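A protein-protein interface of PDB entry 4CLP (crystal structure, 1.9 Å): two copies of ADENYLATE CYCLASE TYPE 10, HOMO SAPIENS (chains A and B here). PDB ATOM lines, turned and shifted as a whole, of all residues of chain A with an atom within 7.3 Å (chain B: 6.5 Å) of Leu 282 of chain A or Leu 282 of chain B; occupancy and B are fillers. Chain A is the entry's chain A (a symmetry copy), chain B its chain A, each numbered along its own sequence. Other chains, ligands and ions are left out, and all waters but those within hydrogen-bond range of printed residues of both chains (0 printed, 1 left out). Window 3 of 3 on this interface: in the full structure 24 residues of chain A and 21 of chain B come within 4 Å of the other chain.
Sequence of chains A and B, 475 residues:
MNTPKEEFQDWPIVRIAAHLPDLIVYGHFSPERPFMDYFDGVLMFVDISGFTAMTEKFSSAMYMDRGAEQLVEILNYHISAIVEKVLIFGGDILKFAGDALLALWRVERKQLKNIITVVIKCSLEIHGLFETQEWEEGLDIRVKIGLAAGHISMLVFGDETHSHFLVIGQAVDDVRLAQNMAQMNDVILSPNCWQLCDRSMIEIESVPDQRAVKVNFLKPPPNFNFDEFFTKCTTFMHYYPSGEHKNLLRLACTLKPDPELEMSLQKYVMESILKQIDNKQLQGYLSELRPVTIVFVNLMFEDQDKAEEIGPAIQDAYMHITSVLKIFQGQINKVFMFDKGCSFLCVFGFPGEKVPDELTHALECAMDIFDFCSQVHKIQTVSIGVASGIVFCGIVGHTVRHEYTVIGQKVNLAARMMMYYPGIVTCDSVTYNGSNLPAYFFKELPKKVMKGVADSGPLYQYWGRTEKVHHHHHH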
ATOM      1  N   LYS A 275      23.767 -21.464  16.530  1.00  0.00           N
ATOM      2  CA  LYS A 275      24.068 -21.403  15.095  1.00  0.00           C
ATOM      3  C   LYS A 275      22.808 -21.124  14.261  1.00  0.00           C
ATOM      4  O   LYS A 275      22.832 -20.326  13.322  1.00  0.00           O
ATOM      5  CB  LYS A 275      24.703 -22.725  14.661  1.00  0.00           C
ATOM      6  CG  LYS A 275      25.624 -22.549  13.500  1.00  0.00           C
ATOM      7  CD  LYS A 275      26.241 -23.915  13.093  1.00  0.00           C
ATOM      8  CE  LYS A 275      26.925 -23.727  11.727  1.00  0.00           C
ATOM      9  NZ  LYS A 275      27.574 -25.006  11.398  1.00  0.00           N
ATOM     10  N   GLN A 276      21.712 -21.784  14.623  1.00  0.00           N
ATOM     11  CA  GLN A 276      20.429 -21.575  13.957  1.00  0.00           C
ATOM     12  C   GLN A 276      19.851 -20.217  14.194  1.00  0.00           C
ATOM     13  O   GLN A 276      19.436 -19.528  13.302  1.00  0.00           O
ATOM     14  CB  GLN A 276      19.487 -22.635  14.417  1.00  0.00           C
ATOM     15  CG  GLN A 276      18.124 -22.323  13.897  1.00  0.00           C
ATOM     16  CD  GLN A 276      17.164 -23.158  14.711  1.00  0.00           C
ATOM     17  OE1 GLN A 276      17.141 -24.437  14.576  1.00  0.00           O
ATOM     18  NE2 GLN A 276      16.492 -22.486  15.697  1.00  0.00           N
ATOM     19  N   ASN A 279      21.346 -17.607  11.963  1.00  0.00           N
ATOM     20  CA  ASN A 279      21.130 -17.897  10.499  1.00  0.00           C
ATOM     21  C   ASN A 279      22.334 -18.420   9.783  1.00  0.00           C
ATOM     22  O   ASN A 279      22.624 -18.064   8.670  1.00  0.00           O
ATOM     23  CB  ASN A 279      20.605 -16.663   9.810  1.00  0.00           C
ATOM     24  CG  ASN A 279      19.378 -16.103  10.449  1.00  0.00           C
ATOM     25  OD1 ASN A 279      18.476 -16.812  10.870  1.00  0.00           O
ATOM     26  ND2 ASN A 279      19.328 -14.801  10.528  1.00  0.00           N
ATOM     27  N   LYS A 280      23.043 -19.285  10.451  1.00  0.00           N
ATOM     28  CA  LYS A 280      24.163 -20.029   9.921  1.00  0.00           C
ATOM     29  C   LYS A 280      23.862 -21.509   9.698  1.00  0.00           C
ATOM     30  O   LYS A 280      24.733 -22.246   9.297  1.00  0.00           O
ATOM     31  CB  LYS A 280      25.414 -19.878  10.853  1.00  0.00           C
ATOM     32  CG  LYS A 280      26.094 -18.516  10.743  1.00  0.00           C
ATOM     33  CD  LYS A 280      27.271 -18.482  11.710  1.00  0.00           C
ATOM     34  CE  LYS A 280      28.413 -17.627  11.204  1.00  0.00           C
ATOM     35  NZ  LYS A 280      27.939 -16.333  10.640  1.00  0.00           N
ATOM     36  N   GLN A 281      22.621 -21.936   9.935  1.00  0.00           N
ATOM     37  CA  GLN A 281      22.212 -23.306   9.687  1.00  0.00           C
ATOM     38  C   GLN A 281      20.719 -23.274   9.454  1.00  0.00           C
ATOM     39  O   GLN A 281      20.015 -22.497  10.069  1.00  0.00           O
ATOM     40  CB  GLN A 281      22.583 -24.132  10.950  1.00  0.00           C
ATOM     41  CG  GLN A 281      22.099 -25.542  11.180  1.00  0.00           C
ATOM     42  CD  GLN A 281      22.528 -25.970  12.632  1.00  0.00           C
ATOM     43  OE1 GLN A 281      23.700 -26.197  12.870  1.00  0.00           O
ATOM     44  NE2 GLN A 281      21.604 -25.927  13.605  1.00  0.00           N
ATOM     45  N   LEU A 282      20.236 -24.150   8.605  1.00  0.00           N
ATOM     46  CA  LEU A 282      18.786 -24.229   8.316  1.00  0.00           C
ATOM     47  C   LEU A 282      18.020 -24.746   9.516  1.00  0.00           C
ATOM     48  O   LEU A 282      18.549 -25.641  10.173  1.00  0.00           O
ATOM     49  CB  LEU A 282      18.665 -25.195   7.169  1.00  0.00           C
ATOM     50  CG  LEU A 282      19.281 -24.731   5.865  1.00  0.00           C
ATOM     51  CD1 LEU A 282      19.597 -25.850   4.889  1.00  0.00           C
ATOM     52  CD2 LEU A 282      18.373 -23.694   5.277  1.00  0.00           C
ATOM     53  N   GLN A 283      16.833 -24.208   9.779  1.00  0.00           N
ATOM     54  CA  GLN A 283      15.954 -24.553  10.942  1.00  0.00           C
ATOM     55  C   GLN A 283      15.662 -26.086  10.904  1.00  0.00           C
ATOM     56  O   GLN A 283      15.712 -26.802  11.882  1.00  0.00           O
ATOM     57  CB  GLN A 283      14.645 -23.747  10.945  1.00  0.00           C
ATOM     58  CG  GLN A 283      14.677 -22.207  10.753  1.00  0.00           C
ATOM     59  CD  GLN A 283      15.335 -21.389  11.910  1.00  0.00           C
ATOM     60  OE1 GLN A 283      15.086 -21.649  13.086  1.00  0.00           O
ATOM     61  NE2 GLN A 283      16.165 -20.378  11.565  1.00  0.00           N
ATOM     62  N   GLY A 284      15.483 -26.614   9.728  1.00  0.00           N
ATOM     63  CA  GLY A 284      15.076 -27.957   9.614  1.00  0.00           C
ATOM     64  C   GLY A 284      15.947 -28.948  10.283  1.00  0.00           C
ATOM     65  O   GLY A 284      15.441 -30.000  10.637  1.00  0.00           O
ATOM     66  N   TYR A 285      17.264 -28.710  10.379  1.00  0.00           N
ATOM     67  CA  TYR A 285      18.104 -29.822  10.672  1.00  0.00           C
ATOM     68  C   TYR A 285      18.106 -30.170  12.138  1.00  0.00           C
ATOM     69  O   TYR A 285      18.553 -31.185  12.460  1.00  0.00           O
ATOM     70  CB  TYR A 285      19.544 -29.678  10.093  1.00  0.00           C
ATOM     71  CG  TYR A 285      19.528 -30.091   8.579  1.00  0.00           C
ATOM     72  CD1 TYR A 285      19.347 -31.439   8.193  1.00  0.00           C
ATOM     73  CD2 TYR A 285      19.564 -29.115   7.547  1.00  0.00           C
ATOM     74  CE1 TYR A 285      19.303 -31.806   6.858  1.00  0.00           C
ATOM     75  CE2 TYR A 285      19.498 -29.487   6.198  1.00  0.00           C
ATOM     76  CZ  TYR A 285      19.377 -30.823   5.872  1.00  0.00           C
ATOM     77  OH  TYR A 285      19.325 -31.194   4.553  1.00  0.00           O
ATOM     78  N   LEU A 286      17.596 -29.349  13.038  1.00  0.00           N
ATOM     79  CA  LEU A 286      17.520 -29.797  14.378  1.00  0.00           C
ATOM     80  C   LEU A 286      16.360 -30.692  14.756  1.00  0.00           C
ATOM     81  O   LEU A 286      16.423 -31.215  15.858  1.00  0.00           O
ATOM     82  CB  LEU A 286      17.597 -28.649  15.356  1.00  0.00           C
ATOM     83  CG  LEU A 286      19.007 -28.052  15.598  1.00  0.00           C
ATOM     84  CD1 LEU A 286      18.861 -26.916  16.555  1.00  0.00           C
ATOM     85  CD2 LEU A 286      19.958 -29.042  16.220  1.00  0.00           C
ATOM     86  N   SER A 287      15.370 -30.922  13.891  1.00  0.00           N
ATOM     87  CA  SER A 287      14.254 -31.838  14.157  1.00  0.00           C
ATOM     88  C   SER A 287      14.624 -33.121  13.544  1.00  0.00           C
ATOM     89  O   SER A 287      14.744 -33.200  12.326  1.00  0.00           O
ATOM     90  CB  SER A 287      12.956 -31.375  13.490  1.00  0.00           C
ATOM     91  OG  SER A 287      12.545 -30.222  14.211  1.00  0.00           O
ATOM     92  N   GLN B 276      12.151 -28.280   1.137  1.00  0.00           N
ATOM     93  CA  GLN B 276      12.107 -26.832   1.319  1.00  0.00           C
ATOM     94  C   GLN B 276      11.084 -26.389   2.316  1.00  0.00           C
ATOM     95  O   GLN B 276      11.337 -25.617   3.199  1.00  0.00           O
ATOM     96  CB  GLN B 276      11.853 -26.202  -0.008  1.00  0.00           C
ATOM     97  CG  GLN B 276      11.614 -24.743   0.191  1.00  0.00           C
ATOM     98  CD  GLN B 276      10.967 -24.247  -1.080  1.00  0.00           C
ATOM     99  OE1 GLN B 276      11.643 -24.191  -2.173  1.00  0.00           O
ATOM    100  NE2 GLN B 276       9.613 -24.058  -1.014  1.00  0.00           N
ATOM    101  N   ASN B 279      12.281 -26.721   5.849  1.00  0.00           N
ATOM    102  CA  ASN B 279      13.511 -25.896   6.128  1.00  0.00           C
ATOM    103  C   ASN B 279      14.783 -26.678   6.199  1.00  0.00           C
ATOM    104  O   ASN B 279      15.633 -26.450   7.021  1.00  0.00           O
ATOM    105  CB  ASN B 279      13.313 -25.101   7.394  1.00  0.00           C
ATOM    106  CG  ASN B 279      12.078 -24.264   7.382  1.00  0.00           C
ATOM    107  OD1 ASN B 279      11.714 -23.648   6.393  1.00  0.00           O
ATOM    108  ND2 ASN B 279      11.409 -24.230   8.503  1.00  0.00           N
ATOM    109  N   LYS B 280      14.903 -27.622   5.309  1.00  0.00           N
ATOM    110  CA  LYS B 280      16.092 -28.414   5.091  1.00  0.00           C
ATOM    111  C   LYS B 280      16.823 -28.073   3.795  1.00  0.00           C
ATOM    112  O   LYS B 280      17.811 -28.697   3.480  1.00  0.00           O
ATOM    113  CB  LYS B 280      15.748 -29.944   5.118  1.00  0.00           C
ATOM    114  CG  LYS B 280      15.483 -30.483   6.521  1.00  0.00           C
ATOM    115  CD  LYS B 280      15.133 -31.963   6.412  1.00  0.00           C
ATOM    116  CE  LYS B 280      15.593 -32.757   7.617  1.00  0.00           C
ATOM    117  NZ  LYS B 280      15.285 -32.061   8.896  1.00  0.00           N
ATOM    118  N   GLN B 281      16.353 -27.066   3.060  1.00  0.00           N
ATOM    119  CA  GLN B 281      17.014 -26.615   1.850  1.00  0.00           C
ATOM    120  C   GLN B 281      16.619 -25.168   1.657  1.00  0.00           C
ATOM    121  O   GLN B 281      15.505 -24.787   1.958  1.00  0.00           O
ATOM    122  CB  GLN B 281      16.506 -27.511   0.686  1.00  0.00           C
ATOM    123  CG  GLN B 281      16.771 -27.201  -0.766  1.00  0.00           C
ATOM    124  CD  GLN B 281      15.953 -28.226  -1.637  1.00  0.00           C
ATOM    125  OE1 GLN B 281      16.310 -29.389  -1.688  1.00  0.00           O
ATOM    126  NE2 GLN B 281      14.797 -27.815  -2.179  1.00  0.00           N
ATOM    127  N   LEU B 282      17.515 -24.380   1.112  1.00  0.00           N
ATOM    128  CA  LEU B 282      17.233 -22.950   0.852  1.00  0.00           C
ATOM    129  C   LEU B 282      16.205 -22.790  -0.248  1.00  0.00           C
ATOM    130  O   LEU B 282      16.277 -23.569  -1.197  1.00  0.00           O
ATOM    131  CB  LEU B 282      18.548 -22.360   0.422  1.00  0.00           C
ATOM    132  CG  LEU B 282      19.627 -22.341   1.485  1.00  0.00           C
ATOM    133  CD1 LEU B 282      21.039 -22.221   0.942  1.00  0.00           C
ATOM    134  CD2 LEU B 282      19.290 -21.249   2.454  1.00  0.00           C
ATOM    135  N   GLN B 283      15.298 -21.826  -0.122  1.00  0.00           N
ATOM    136  CA  GLN B 283      14.179 -21.545  -1.078  1.00  0.00           C
ATOM    137  C   GLN B 283      14.789 -21.293  -2.492  1.00  0.00           C
ATOM    138  O   GLN B 283      14.340 -21.777  -3.511  1.00  0.00           O
ATOM    139  CB  GLN B 283      13.315 -20.355  -0.634  1.00  0.00           C
ATOM    140  CG  GLN B 283      12.789 -20.272   0.824  1.00  0.00           C
ATOM    141  CD  GLN B 283      11.737 -21.353   1.232  1.00  0.00           C
ATOM    142  OE1 GLN B 283      10.810 -21.643   0.478  1.00  0.00           O
ATOM    143  NE2 GLN B 283      11.878 -21.932   2.446  1.00  0.00           N
ATOM    144  N   GLY B 284      15.908 -20.631  -2.532  1.00  0.00           N
ATOM    145  CA  GLY B 284      16.450 -20.239  -3.772  1.00  0.00           C
ATOM    146  C   GLY B 284      16.687 -21.332  -4.741  1.00  0.00           C
ATOM    147  O   GLY B 284      16.681 -21.049  -5.927  1.00  0.00           O
ATOM    148  N   TYR B 285      17.003 -22.556  -4.289  1.00  0.00           N
ATOM    149  CA  TYR B 285      17.587 -23.460  -5.223  1.00  0.00           C
ATOM    150  C   TYR B 285      16.559 -24.104  -6.118  1.00  0.00           C
ATOM    151  O   TYR B 285      16.927 -24.665  -7.058  1.00  0.00           O
ATOM    152  CB  TYR B 285      18.538 -24.501  -4.562  1.00  0.00           C
ATOM    153  CG  TYR B 285      19.940 -23.837  -4.330  1.00  0.00           C
ATOM    154  CD1 TYR B 285      20.790 -23.531  -5.418  1.00  0.00           C
ATOM    155  CD2 TYR B 285      20.349 -23.404  -3.041  1.00  0.00           C
ATOM    156  CE1 TYR B 285      22.017 -22.918  -5.223  1.00  0.00           C
ATOM    157  CE2 TYR B 285      21.581 -22.766  -2.849  1.00  0.00           C
ATOM    158  CZ  TYR B 285      22.399 -22.539  -3.937  1.00  0.00           C
ATOM    159  OH  TYR B 285      23.612 -21.927  -3.754  1.00  0.00           O
ATOM    160  N   LEU B 286      15.269 -24.020  -5.850  1.00  0.00           N
ATOM    161  CA  LEU B 286      14.360 -24.542  -6.800  1.00  0.00           C
ATOM    162  C   LEU B 286      14.015 -23.677  -7.993  1.00  0.00           C
ATOM    163  O   LEU B 286      13.385 -24.221  -8.886  1.00  0.00           O
ATOM    164  CB  LEU B 286      13.081 -25.015  -6.148  1.00  0.00           C
ATOM    165  CG  LEU B 286      13.154 -26.380  -5.416  1.00  0.00           C
ATOM    166  CD1 LEU B 286      11.815 -26.644  -4.814  1.00  0.00           C
ATOM    167  CD2 LEU B 286      13.459 -27.525  -6.349  1.00  0.00           C
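N of Gly 284 of chain A is in hydrogen-bond range of O of Asn 279 of chain B (2.7 Å). The side-chain amino group (NZ) of Lys 280 of chain B is in hydrogen-bond range of the backbone carbonyl oxygen (O) of Gly 284 of chain A. The backbone carbonyl oxygen of Lys 280 of chain B sits at hydrogen-bond distance from the side-chain hydroxyl of Tyr 285 of chain A, at 3.1 Å.
The side-chain amide oxygen of Gln 283 of chain A sits close to the side-chain amide nitrogen of Gln 276 of chain A (3.1 Å).
Among the printed residues, merely in contact across the chains: Leu 282 of chain A with Asn 279 of chain B (3.3 Å), Leu 282 of chain A with Lys 280 of chain B (3.6 Å), Leu 282 of chain A with Gln 281 of chain B (3.9 Å), Leu 282 of chain A with Leu 282 of chain B (3.8 Å), Gln 283 of chain A with Asn 279 of chain B (3.8 Å) and Ser 287 of chain A with Lys 280 of chain B (3.7 Å).
Of chain B, only Asn 279, Lys 280, Gln 281 and Leu 282 come within 4 Å of Leu 282 of chain A. Of the printed residues of chain A, Leu 282 of chain B touches Leu 282. Printed residues of chain B within 4 Å of Ser 287 of chain A: Lys 280. Of the printed residues of chain A, Gln 281 of chain B touches Leu 282. Of the printed residues of chain A, Lys 280 of chain B touches Leu 282, Gly 284, Tyr 285 and Ser 287. Gln 283 of chain B touches none of the printed residues of chain A. The nearest printed residue of chain B that does not touch Leu 282 of chain A is Gln 283 of chain B (6.5 Å). The nearest printed residue of chain B that does not touch Gln 283 of chain A is Lys 280 of chain B (5.9 Å).
Of the 11 printed residues of chain A, 5 touch a printed residue of chain B. Of the 9 printed residues of chain B, 4 touch a printed residue of chain A. Printed residues of chain B that touch a printed residue of chain A: Asn 279, Lys 280, Gln 281 and Leu 282. Hydrophobic or aromatic side chains of chain B that line the printed part of chain A: Leu 282. Along chain B the printed residues that touch a printed residue of chain A span positions 279 to 282. Among the printed residues, no Asp or Glu carboxylate lies within 4 Å of a Lys or Arg side-chain nitrogen of the other chain.
Leu 282 of chain A touches Asn 279 of chain B, but with the chains exchanged Asn 279 of chain A does not touch Leu 282 of chain B (7.7 Å). Leu 282 of chain A touches Lys 280 of chain B, but with the chains exchanged Lys 280 of chain A does not touch Leu 282 of chain B (8.6 Å). Gly 284 of chain A touches Asn 279 of chain B, but with the chains exchanged Asn 279 of chain A does not touch Gly 284 of chain B (13.3 Å). Tyr 285 of chain A touches Lys 280 of chain B, but with the chains exchanged Lys 280 of chain A does not touch Tyr 285 of chain B (12.6 Å). Of the 9 pairs that touch across the chains among the printed residues, 1 has its exchanged pair printed and touching as well.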
